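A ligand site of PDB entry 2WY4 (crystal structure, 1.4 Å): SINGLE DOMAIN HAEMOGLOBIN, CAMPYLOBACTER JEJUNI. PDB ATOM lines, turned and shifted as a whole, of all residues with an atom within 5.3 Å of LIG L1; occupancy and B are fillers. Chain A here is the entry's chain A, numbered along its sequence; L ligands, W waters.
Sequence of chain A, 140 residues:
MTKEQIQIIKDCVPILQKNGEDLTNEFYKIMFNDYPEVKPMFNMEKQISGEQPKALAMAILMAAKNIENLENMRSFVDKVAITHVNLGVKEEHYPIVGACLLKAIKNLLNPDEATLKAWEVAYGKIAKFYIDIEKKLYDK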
ATOM      1  N   MET A  31     -12.616  -5.214  -2.512  1.00  0.00           N
ATOM      2  CA  MET A  31     -12.919  -6.581  -2.219  1.00  0.00           C
ATOM      3  C   MET A  31     -11.944  -7.214  -1.241  1.00  0.00           C
ATOM      4  O   MET A  31     -12.341  -7.898  -0.325  1.00  0.00           O
ATOM      5  CB  MET A  31     -13.065  -7.443  -3.445  1.00  0.00           C
ATOM      6  CG  MET A  31     -13.566  -8.848  -3.139  1.00  0.00           C
ATOM      7  SD  MET A  31     -14.075  -9.766  -4.601  1.00  0.00           S
ATOM      8  CE  MET A  31     -12.525  -9.891  -5.478  1.00  0.00           C
ATOM      9  N   VAL A  38     -11.402 -13.919   0.533  1.00  0.00           N
ATOM     10  CA  VAL A  38     -11.272 -14.339  -0.873  1.00  0.00           C
ATOM     11  C   VAL A  38      -9.884 -14.083  -1.429  1.00  0.00           C
ATOM     12  O   VAL A  38      -9.529 -14.669  -2.441  1.00  0.00           O
ATOM     13  CB  VAL A  38     -12.346 -13.705  -1.826  1.00  0.00           C
ATOM     14  CG1 VAL A  38     -13.740 -13.876  -1.275  1.00  0.00           C
ATOM     15  CG2 VAL A  38     -12.027 -12.251  -2.103  1.00  0.00           C
ATOM     16  N   MET A  41      -7.476 -16.801  -2.983  1.00  0.00           N
ATOM     17  CA  MET A  41      -7.919 -17.432  -4.210  1.00  0.00           C
ATOM     18  C   MET A  41      -7.158 -16.838  -5.414  1.00  0.00           C
ATOM     19  O   MET A  41      -6.891 -17.533  -6.420  1.00  0.00           O
ATOM     20  CB  MET A  41      -9.402 -17.200  -4.408  1.00  0.00           C
ATOM     21  CG  MET A  41     -10.278 -17.826  -3.343  1.00  0.00           C
ATOM     22  SD  MET A  41     -12.024 -17.341  -3.452  1.00  0.00           S
ATOM     23  CE  MET A  41     -12.634 -18.294  -4.766  1.00  0.00           C
ATOM     24  N   PHE A  42      -6.772 -15.583  -5.295  1.00  0.00           N
ATOM     25  CA  PHE A  42      -6.116 -14.845  -6.358  1.00  0.00           C
ATOM     26  C   PHE A  42      -4.606 -14.916  -6.234  1.00  0.00           C
ATOM     27  O   PHE A  42      -4.082 -15.082  -5.141  1.00  0.00           O
ATOM     28  CB  PHE A  42      -6.518 -13.371  -6.261  1.00  0.00           C
ATOM     29  CG  PHE A  42      -7.967 -13.124  -6.556  1.00  0.00           C
ATOM     30  CD1 PHE A  42      -8.955 -13.276  -5.581  1.00  0.00           C
ATOM     31  CD2 PHE A  42      -8.347 -12.734  -7.795  1.00  0.00           C
ATOM     32  CE1 PHE A  42     -10.250 -13.076  -5.892  1.00  0.00           C
ATOM     33  CE2 PHE A  42      -9.649 -12.508  -8.081  1.00  0.00           C
ATOM     34  CZ  PHE A  42     -10.620 -12.676  -7.112  1.00  0.00           C
ATOM     35  N   ASN A  43      -3.943 -14.786  -7.373  1.00  0.00           N
ATOM     36  CA  ASN A  43      -2.496 -14.727  -7.388  1.00  0.00           C
ATOM     37  C   ASN A  43      -2.045 -13.281  -7.246  1.00  0.00           C
ATOM     38  O   ASN A  43      -2.265 -12.457  -8.112  1.00  0.00           O
ATOM     39  CB  ASN A  43      -1.974 -15.349  -8.691  1.00  0.00           C
ATOM     40  CG  ASN A  43      -2.257 -16.824  -8.754  1.00  0.00           C
ATOM     41  OD1 ASN A  43      -1.771 -17.601  -7.903  1.00  0.00           O
ATOM     42  ND2 ASN A  43      -3.068 -17.247  -9.726  1.00  0.00           N
ATOM     43  N   LYS A  46      -0.152 -11.555 -10.009  1.00  0.00           N
ATOM     44  CA  LYS A  46      -0.996 -11.111 -11.136  1.00  0.00           C
ATOM     45  C   LYS A  46      -1.704  -9.785 -10.807  1.00  0.00           C
ATOM     46  O   LYS A  46      -2.140  -9.090 -11.721  1.00  0.00           O
ATOM     47  CB  LYS A  46      -2.006 -12.226 -11.524  1.00  0.00           C
ATOM     48  CG  LYS A  46      -2.337 -12.381 -13.022  1.00  0.00           C
ATOM     49  CD  LYS A  46      -3.495 -13.345 -13.288  1.00  0.00           C
ATOM     50  CE  LYS A  46      -4.052 -13.197 -14.678  1.00  0.00           C
ATOM     51  NZ  LYS A  46      -5.385 -13.764 -15.053  1.00  0.00           N
ATOM     52  N   GLN A  52      -4.133  -9.172 -13.829  1.00  0.00           N
ATOM     53  CA  GLN A  52      -5.513  -9.516 -13.466  1.00  0.00           C
ATOM     54  C   GLN A  52      -6.475  -8.311 -13.500  1.00  0.00           C
ATOM     55  O   GLN A  52      -7.575  -8.447 -13.978  1.00  0.00           O
ATOM     56  CB  GLN A  52      -5.539 -10.295 -12.146  1.00  0.00           C
ATOM     57  CG  GLN A  52      -6.957 -10.632 -11.679  1.00  0.00           C
ATOM     58  CD  GLN A  52      -7.625 -11.574 -12.627  1.00  0.00           C
ATOM     59  OE1 GLN A  52      -6.984 -12.349 -13.343  1.00  0.00           O
ATOM     60  NE2 GLN A  52      -8.965 -11.547 -12.616  1.00  0.00           N
ATOM     61  N   ALA A  55      -7.299  -8.060 -17.018  1.00  0.00           N
ATOM     62  CA  ALA A  55      -8.115  -9.150 -17.470  1.00  0.00           C
ATOM     63  C   ALA A  55      -9.587  -8.929 -17.082  1.00  0.00           C
ATOM     64  O   ALA A  55     -10.511  -9.189 -17.863  1.00  0.00           O
ATOM     65  CB  ALA A  55      -7.638 -10.466 -16.908  1.00  0.00           C
ATOM     66  N   LEU A  56      -9.825  -8.501 -15.836  1.00  0.00           N
ATOM     67  CA  LEU A  56     -11.186  -8.257 -15.385  1.00  0.00           C
ATOM     68  C   LEU A  56     -11.799  -7.130 -16.165  1.00  0.00           C
ATOM     69  O   LEU A  56     -12.976  -7.230 -16.554  1.00  0.00           O
ATOM     70  CB  LEU A  56     -11.201  -7.963 -13.897  1.00  0.00           C
ATOM     71  CG  LEU A  56     -12.604  -7.724 -13.323  1.00  0.00           C
ATOM     72  CD1 LEU A  56     -13.545  -8.901 -13.597  1.00  0.00           C
ATOM     73  CD2 LEU A  56     -12.469  -7.395 -11.832  1.00  0.00           C
ATOM     74  N   ALA A  59     -12.874  -8.383 -19.436  1.00  0.00           N
ATOM     75  CA  ALA A  59     -14.071  -9.204 -19.349  1.00  0.00           C
ATOM     76  C   ALA A  59     -15.329  -8.347 -19.152  1.00  0.00           C
ATOM     77  O   ALA A  59     -16.398  -8.718 -19.672  1.00  0.00           O
ATOM     78  CB  ALA A  59     -13.939 -10.157 -18.216  1.00  0.00           C
ATOM     79  N   ILE A  60     -15.222  -7.271 -18.361  1.00  0.00           N
ATOM     80  CA  ILE A  60     -16.348  -6.369 -18.201  1.00  0.00           C
ATOM     81  C   ILE A  60     -16.659  -5.723 -19.542  1.00  0.00           C
ATOM     82  O   ILE A  60     -17.813  -5.594 -19.915  1.00  0.00           O
ATOM     83  CB  ILE A  60     -16.106  -5.357 -17.043  1.00  0.00           C
ATOM     84  CG1 ILE A  60     -15.983  -6.115 -15.719  1.00  0.00           C
ATOM     85  CG2 ILE A  60     -17.261  -4.370 -16.964  1.00  0.00           C
ATOM     86  CD1 ILE A  60     -15.494  -5.282 -14.563  1.00  0.00           C
ATOM     87  N   PHE A  76     -15.919 -17.015 -24.761  1.00  0.00           N
ATOM     88  CA  PHE A  76     -15.018 -16.325 -23.849  1.00  0.00           C
ATOM     89  C   PHE A  76     -15.271 -16.815 -22.420  1.00  0.00           C
ATOM     90  O   PHE A  76     -14.391 -17.222 -21.692  1.00  0.00           O
ATOM     91  CB  PHE A  76     -15.215 -14.797 -23.920  1.00  0.00           C
ATOM     92  CG  PHE A  76     -14.418 -14.038 -22.892  1.00  0.00           C
ATOM     93  CD1 PHE A  76     -13.071 -13.921 -23.014  1.00  0.00           C
ATOM     94  CD2 PHE A  76     -15.037 -13.488 -21.773  1.00  0.00           C
ATOM     95  CE1 PHE A  76     -12.330 -13.283 -22.074  1.00  0.00           C
ATOM     96  CE2 PHE A  76     -14.284 -12.823 -20.841  1.00  0.00           C
ATOM     97  CZ  PHE A  76     -12.939 -12.730 -20.983  1.00  0.00           C
ATOM     98  N   LYS A  79     -14.159 -20.214 -21.066  1.00  0.00           N
ATOM     99  CA  LYS A  79     -12.770 -20.353 -20.665  1.00  0.00           C
ATOM    100  C   LYS A  79     -12.518 -19.766 -19.293  1.00  0.00           C
ATOM    101  O   LYS A  79     -11.754 -20.359 -18.508  1.00  0.00           O
ATOM    102  CB  LYS A  79     -11.846 -19.679 -21.663  1.00  0.00           C
ATOM    103  CG  LYS A  79     -12.062 -20.125 -23.088  1.00  0.00           C
ATOM    104  CD  LYS A  79     -12.206 -21.627 -23.201  1.00  0.00           C
ATOM    105  CE  LYS A  79     -12.455 -22.071 -24.625  1.00  0.00           C
ATOM    106  NZ  LYS A  79     -13.798 -21.630 -25.163  1.00  0.00           N
ATOM    107  N   VAL A  80     -13.141 -18.627 -18.997  1.00  0.00           N
ATOM    108  CA  VAL A  80     -12.980 -18.040 -17.676  1.00  0.00           C
ATOM    109  C   VAL A  80     -13.567 -19.012 -16.625  1.00  0.00           C
ATOM    110  O   VAL A  80     -13.004 -19.184 -15.567  1.00  0.00           O
ATOM    111  CB  VAL A  80     -13.700 -16.701 -17.539  1.00  0.00           C
ATOM    112  CG1 VAL A  80     -13.558 -16.188 -16.123  1.00  0.00           C
ATOM    113  CG2 VAL A  80     -13.143 -15.680 -18.547  1.00  0.00           C
ATOM    114  N   THR A  83     -11.200 -21.360 -14.823  1.00  0.00           N
ATOM    115  CA  THR A  83     -10.447 -20.790 -13.726  1.00  0.00           C
ATOM    116  C   THR A  83     -11.296 -20.696 -12.469  1.00  0.00           C
ATOM    117  O   THR A  83     -10.904 -21.127 -11.383  1.00  0.00           O
ATOM    118  CB  THR A  83      -9.974 -19.393 -14.112  1.00  0.00           C
ATOM    119  OG1 THR A  83      -9.013 -19.511 -15.152  1.00  0.00           O
ATOM    120  CG2 THR A  83      -9.296 -18.676 -12.951  1.00  0.00           C
ATOM    121  N   HIS A  84     -12.490 -20.165 -12.645  1.00  0.00           N
ATOM    122  CA  HIS A  84     -13.389 -19.983 -11.514  1.00  0.00           C
ATOM    123  C   HIS A  84     -13.736 -21.310 -10.833  1.00  0.00           C
ATOM    124  O   HIS A  84     -13.651 -21.414  -9.603  1.00  0.00           O
ATOM    125  CB  HIS A  84     -14.658 -19.321 -12.020  1.00  0.00           C
ATOM    126  CG  HIS A  84     -14.542 -17.842 -12.240  1.00  0.00           C
ATOM    127  ND1 HIS A  84     -15.548 -17.099 -12.842  1.00  0.00           N
ATOM    128  CD2 HIS A  84     -13.555 -16.971 -11.937  1.00  0.00           C
ATOM    129  CE1 HIS A  84     -15.192 -15.824 -12.860  1.00  0.00           C
ATOM    130  NE2 HIS A  84     -13.972 -15.724 -12.334  1.00  0.00           N
ATOM    131  N   LEU A  87     -10.858 -22.810  -8.906  1.00  0.00           N
ATOM    132  CA  LEU A  87     -10.518 -22.088  -7.684  1.00  0.00           C
ATOM    133  C   LEU A  87     -11.640 -22.046  -6.637  1.00  0.00           C
ATOM    134  O   LEU A  87     -11.483 -21.448  -5.583  1.00  0.00           O
ATOM    135  CB  LEU A  87     -10.067 -20.670  -8.028  1.00  0.00           C
ATOM    136  CG  LEU A  87      -8.654 -20.664  -8.638  1.00  0.00           C
ATOM    137  CD1 LEU A  87      -8.271 -19.299  -9.158  1.00  0.00           C
ATOM    138  CD2 LEU A  87      -7.608 -21.167  -7.611  1.00  0.00           C
ATOM    139  N   VAL A  89     -14.829 -20.846  -6.998  1.00  0.00           N
ATOM    140  CA  VAL A  89     -15.775 -19.739  -7.070  1.00  0.00           C
ATOM    141  C   VAL A  89     -17.171 -20.336  -7.056  1.00  0.00           C
ATOM    142  O   VAL A  89     -17.537 -21.174  -7.884  1.00  0.00           O
ATOM    143  CB  VAL A  89     -15.573 -18.951  -8.350  1.00  0.00           C
ATOM    144  CG1 VAL A  89     -16.660 -17.924  -8.512  1.00  0.00           C
ATOM    145  CG2 VAL A  89     -14.181 -18.313  -8.382  1.00  0.00           C
ATOM    146  N   LYS A  90     -17.998 -19.874  -6.119  1.00  0.00           N
ATOM    147  CA  LYS A  90     -19.362 -20.353  -5.996  1.00  0.00           C
ATOM    148  C   LYS A  90     -20.376 -19.305  -6.361  1.00  0.00           C
ATOM    149  O   LYS A  90     -20.073 -18.112  -6.378  1.00  0.00           O
ATOM    150  CB  LYS A  90     -19.664 -20.797  -4.563  1.00  0.00           C
ATOM    151  CG  LYS A  90     -18.697 -21.793  -4.007  1.00  0.00           C
ATOM    152  CD  LYS A  90     -18.784 -23.100  -4.748  1.00  0.00           C
ATOM    153  CE  LYS A  90     -17.623 -24.005  -4.365  1.00  0.00           C
ATOM    154  NZ  LYS A  90     -17.754 -25.368  -4.929  1.00  0.00           N
ATOM    155  N   HIS A  93     -20.498 -16.265  -4.244  1.00  0.00           N
ATOM    156  CA  HIS A  93     -19.463 -15.208  -4.282  1.00  0.00           C
ATOM    157  C   HIS A  93     -19.872 -14.088  -5.215  1.00  0.00           C
ATOM    158  O   HIS A  93     -19.408 -13.001  -5.080  1.00  0.00           O
ATOM    159  CB  HIS A  93     -18.133 -15.728  -4.803  1.00  0.00           C
ATOM    160  CG  HIS A  93     -17.378 -16.609  -3.854  1.00  0.00           C
ATOM    161  ND1 HIS A  93     -17.082 -17.921  -4.142  1.00  0.00           N
ATOM    162  CD2 HIS A  93     -16.826 -16.349  -2.639  1.00  0.00           C
ATOM    163  CE1 HIS A  93     -16.400 -18.433  -3.127  1.00  0.00           C
ATOM    164  NE2 HIS A  93     -16.209 -17.490  -2.223  1.00  0.00           N
ATOM    165  N   TYR A  94     -20.762 -14.368  -6.154  1.00  0.00           N
ATOM    166  CA  TYR A  94     -21.141 -13.356  -7.140  1.00  0.00           C
ATOM    167  C   TYR A  94     -21.773 -12.093  -6.518  1.00  0.00           C
ATOM    168  O   TYR A  94     -21.462 -10.996  -6.988  1.00  0.00           O
ATOM    169  CB  TYR A  94     -21.947 -13.933  -8.321  1.00  0.00           C
ATOM    170  CG  TYR A  94     -21.085 -14.666  -9.307  1.00  0.00           C
ATOM    171  CD1 TYR A  94     -20.710 -15.966  -9.082  1.00  0.00           C
ATOM    172  CD2 TYR A  94     -20.582 -14.020 -10.437  1.00  0.00           C
ATOM    173  CE1 TYR A  94     -19.874 -16.627  -9.951  1.00  0.00           C
ATOM    174  CE2 TYR A  94     -19.754 -14.666 -11.303  1.00  0.00           C
ATOM    175  CZ  TYR A  94     -19.406 -15.963 -11.065  1.00  0.00           C
ATOM    176  OH  TYR A  94     -18.588 -16.632 -11.948  1.00  0.00           O
ATOM    177  N   VAL A  97     -18.803  -9.880  -5.359  1.00  0.00           N
ATOM    178  CA  VAL A  97     -18.222  -9.183  -6.500  1.00  0.00           C
ATOM    179  C   VAL A  97     -19.117  -8.038  -6.963  1.00  0.00           C
ATOM    180  O   VAL A  97     -18.630  -6.944  -7.250  1.00  0.00           O
ATOM    181  CB  VAL A  97     -17.859 -10.185  -7.653  1.00  0.00           C
ATOM    182  CG1 VAL A  97     -17.610  -9.467  -8.958  1.00  0.00           C
ATOM    183  CG2 VAL A  97     -16.656 -11.009  -7.226  1.00  0.00           C
ATOM    184  N   TYR A 123     -25.091  -6.150 -14.172  1.00  0.00           N
ATOM    185  CA  TYR A 123     -24.295  -7.090 -13.403  1.00  0.00           C
ATOM    186  C   TYR A 123     -25.108  -8.342 -13.038  1.00  0.00           C
ATOM    187  O   TYR A 123     -24.625  -9.455 -13.119  1.00  0.00           O
ATOM    188  CB  TYR A 123     -23.693  -6.482 -12.117  1.00  0.00           C
ATOM    189  CG  TYR A 123     -22.882  -7.534 -11.385  1.00  0.00           C
ATOM    190  CD1 TYR A 123     -21.575  -7.834 -11.796  1.00  0.00           C
ATOM    191  CD2 TYR A 123     -23.444  -8.314 -10.395  1.00  0.00           C
ATOM    192  CE1 TYR A 123     -20.857  -8.804 -11.208  1.00  0.00           C
ATOM    193  CE2 TYR A 123     -22.714  -9.296  -9.779  1.00  0.00           C
ATOM    194  CZ  TYR A 123     -21.424  -9.562 -10.210  1.00  0.00           C
ATOM    195  OH  TYR A 123     -20.702 -10.573  -9.604  1.00  0.00           O
ATOM    196  N   ILE A 126     -25.056 -10.520 -16.112  1.00  0.00           N
ATOM    197  CA  ILE A 126     -23.731 -11.024 -16.436  1.00  0.00           C
ATOM    198  C   ILE A 126     -23.371 -12.121 -15.449  1.00  0.00           C
ATOM    199  O   ILE A 126     -22.940 -13.206 -15.807  1.00  0.00           O
ATOM    200  CB  ILE A 126     -22.746  -9.865 -16.348  1.00  0.00           C
ATOM    201  CG1 ILE A 126     -22.999  -8.858 -17.442  1.00  0.00           C
ATOM    202  CG2 ILE A 126     -21.317 -10.374 -16.477  1.00  0.00           C
ATOM    203  CD1 ILE A 126     -22.322  -7.541 -17.194  1.00  0.00           C
ATOM    204  N   ALA A 127     -23.647 -11.871 -14.170  1.00  0.00           N
ATOM    205  CA  ALA A 127     -23.383 -12.852 -13.154  1.00  0.00           C
ATOM    206  C   ALA A 127     -24.143 -14.130 -13.420  1.00  0.00           C
ATOM    207  O   ALA A 127     -23.596 -15.198 -13.260  1.00  0.00           O
ATOM    208  CB  ALA A 127     -23.702 -12.310 -11.777  1.00  0.00           C
ATOM    209  N   TYR A 130     -22.438 -16.262 -16.096  1.00  0.00           N
ATOM    210  CA  TYR A 130     -21.271 -16.974 -15.582  1.00  0.00           C
ATOM    211  C   TYR A 130     -21.688 -18.111 -14.648  1.00  0.00           C
ATOM    212  O   TYR A 130     -21.222 -19.258 -14.781  1.00  0.00           O
ATOM    213  CB  TYR A 130     -20.353 -16.031 -14.811  1.00  0.00           C
ATOM    214  CG  TYR A 130     -19.362 -15.257 -15.646  1.00  0.00           C
ATOM    215  CD1 TYR A 130     -19.765 -14.206 -16.435  1.00  0.00           C
ATOM    216  CD2 TYR A 130     -18.003 -15.586 -15.615  1.00  0.00           C
ATOM    217  CE1 TYR A 130     -18.862 -13.495 -17.182  1.00  0.00           C
ATOM    218  CE2 TYR A 130     -17.098 -14.892 -16.378  1.00  0.00           C
ATOM    219  CZ  TYR A 130     -17.510 -13.840 -17.162  1.00  0.00           C
ATOM    220  OH  TYR A 130     -16.551 -13.204 -17.914  1.00  0.00           O
HETATM  221  C1  LIG L   1     -10.124 -14.876 -12.680  1.00  0.00           C
HETATM  222  C2  LIG L   1     -13.683 -12.392 -14.750  1.00  0.00           C
HETATM  223  C3  LIG L   1     -16.419 -13.147 -10.852  1.00  0.00           C
HETATM  224  C4  LIG L   1     -12.605 -15.062  -8.546  1.00  0.00           C
HETATM  225  C5  LIG L   1     -10.858 -14.222 -13.604  1.00  0.00           C
HETATM  226  C6  LIG L   1     -10.449 -13.878 -14.929  1.00  0.00           C
HETATM  227  C7  LIG L   1     -11.429 -13.157 -15.519  1.00  0.00           C
HETATM  228  C8  LIG L   1     -12.484 -13.048 -14.534  1.00  0.00           C
HETATM  229  C9  LIG L   1     -11.426 -12.604 -16.950  1.00  0.00           C
HETATM  230  C10 LIG L   1      -9.092 -14.278 -15.562  1.00  0.00           C
HETATM  231  C11 LIG L   1      -8.977 -15.792 -15.713  1.00  0.00           C
HETATM  232  C12 LIG L   1      -9.371 -16.393 -17.030  1.00  0.00           C
HETATM  233  O1  LIG L   1      -9.491 -15.655 -18.038  1.00  0.00           O
HETATM  234  O2  LIG L   1      -9.489 -17.668 -17.072  1.00  0.00           O
HETATM  235  C13 LIG L   1     -14.722 -12.358 -13.854  1.00  0.00           C
HETATM  236  C14 LIG L   1     -15.981 -11.752 -14.092  1.00  0.00           C
HETATM  237  C15 LIG L   1     -16.748 -11.961 -13.013  1.00  0.00           C
HETATM  238  C16 LIG L   1     -15.992 -12.707 -12.069  1.00  0.00           C
HETATM  239  C17 LIG L   1     -16.336 -10.935 -15.332  1.00  0.00           C
HETATM  240  C18 LIG L   1     -18.176 -11.489 -12.708  1.00  0.00           C
HETATM  241  C19 LIG L   1     -19.144 -11.553 -13.604  1.00  0.00           C
HETATM  242  C20 LIG L   1     -15.673 -13.769  -9.889  1.00  0.00           C
HETATM  243  C21 LIG L   1     -16.076 -14.224  -8.596  1.00  0.00           C
HETATM  244  C22 LIG L   1     -15.011 -14.713  -7.998  1.00  0.00           C
HETATM  245  C23 LIG L   1     -13.866 -14.578  -8.851  1.00  0.00           C
HETATM  246  C24 LIG L   1     -17.518 -14.190  -8.079  1.00  0.00           C
HETATM  247  C25 LIG L   1     -14.980 -15.309  -6.603  1.00  0.00           C
HETATM  248  C26 LIG L   1     -14.195 -14.753  -5.670  1.00  0.00           C
HETATM  249  C27 LIG L   1     -11.596 -15.185  -9.483  1.00  0.00           C
HETATM  250  C28 LIG L   1     -10.323 -15.712  -9.165  1.00  0.00           C
HETATM  251  C29 LIG L   1      -9.524 -15.681 -10.416  1.00  0.00           C
HETATM  252  C30 LIG L   1     -10.415 -15.130 -11.388  1.00  0.00           C
HETATM  253  C31 LIG L   1      -9.880 -16.228  -7.811  1.00  0.00           C
HETATM  254  C32 LIG L   1      -8.084 -16.101 -10.637  1.00  0.00           C
HETATM  255  C33 LIG L   1      -7.228 -14.843 -10.747  1.00  0.00           C
HETATM  256  C34 LIG L   1      -5.750 -15.093 -10.647  1.00  0.00           C
HETATM  257  O3  LIG L   1      -5.103 -14.345  -9.908  1.00  0.00           O
HETATM  258  O4  LIG L   1      -5.269 -16.027 -11.335  1.00  0.00           O
HETATM  259  N1  LIG L   1     -12.108 -13.709 -13.357  1.00  0.00           N
HETATM  260  N2  LIG L   1     -14.743 -12.948 -12.616  1.00  0.00           N
HETATM  261  N3  LIG L   1     -14.316 -14.004 -10.024  1.00  0.00           N
HETATM  262  N4  LIG L   1     -11.634 -14.831 -10.814  1.00  0.00           N
HETATM  263 FE1  LIG L   1     -13.206 -13.885 -11.718  1.00  0.00          FE
HETATM  264  C1  LG2 L   2     -12.414 -12.173 -11.017  1.00  0.00           C
HETATM  265  N1  LG2 L   2     -11.898 -11.207 -10.675  1.00  0.00           N
HETATM  266  O   HOH W   1      -4.920 -11.845  -9.107  1.00  0.00           O
HETATM  267  O   HOH W   2      -9.398 -16.855 -20.344  1.00  0.00           O
HETATM  268  O   HOH W   3      -8.589 -13.397 -19.151  1.00  0.00           O
HETATM  269  O   HOH W   4      -5.230 -16.551 -13.863  1.00  0.00           O
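The side-chain hydroxyl of Thr 83 sits at hydrogen-bond distance from an oxygen (O2) of LIG L1 (2.7 Å).
FE1 of LIG L1 is bound by NE2 of His 84 (2.1 Å).
O3 of LIG L1 sits at hydrogen-bond distance from N of Asn 43 (2.8 Å).
The side-chain amide nitrogen (ND2) of Asn 43 lies within hydrogen-bond range of an oxygen (O4) of LIG L1, 3.0 Å away.
ND1 of His 93 sits at hydrogen-bond distance from N of Lys 90, at 2.9 Å.
The backbone carbonyl oxygen (O) of His 84 is in hydrogen-bond range of the backbone NH (N) of Val 89.
OE1 of Gln 52 is in hydrogen-bond range of NZ of Lys 46 (2.7 Å).
The backbone carbonyl oxygen (O) of Tyr 94 lies within hydrogen-bond range of the side-chain hydroxyl (OH) of Tyr 123.
ND1 of His 84 sits at hydrogen-bond distance from OH of Tyr 94, 3.2 Å away.
Merely in contact with LIG L1: Val 97, Phe 42, Gln 52, Tyr 130, Leu 87, Met 41, Val 80, Val 89, Ala 55, His 93, Leu 56, Tyr 94, Ala 59, Lys 46, Ile 126 and Lys 79.
Hydrophobic or aromatic side chains that line LIG L1: Met 41, Phe 42, Leu 56, Ala 59, Val 80, His 84, Leu 87, Val 89, His 93, Tyr 94, Val 97, Ile 126 and Tyr 130.
Within 4 Å of LIG L1: Met 41, Phe 42, Asn 43, Lys 46, Gln 52, Ala 55, Leu 56, Ala 59, Lys 79, Val 80, Thr 83, His 84, Leu 87, Val 89, His 93, Tyr 94, Val 97, Ile 126 and Tyr 130.
Along chain A the residues within 4 Å of LIG L1 span positions 41 to 130.
The nearest printed residue that does not touch LIG L1 is Tyr 123 (4.03 Å).
Water W4 bridges O4 of LIG L1 (2.6 Å) and NZ of Lys 46 (3.0 Å).
Water W1 lies within hydrogen-bond range of O3 of LIG L1 and O of Asn 43.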
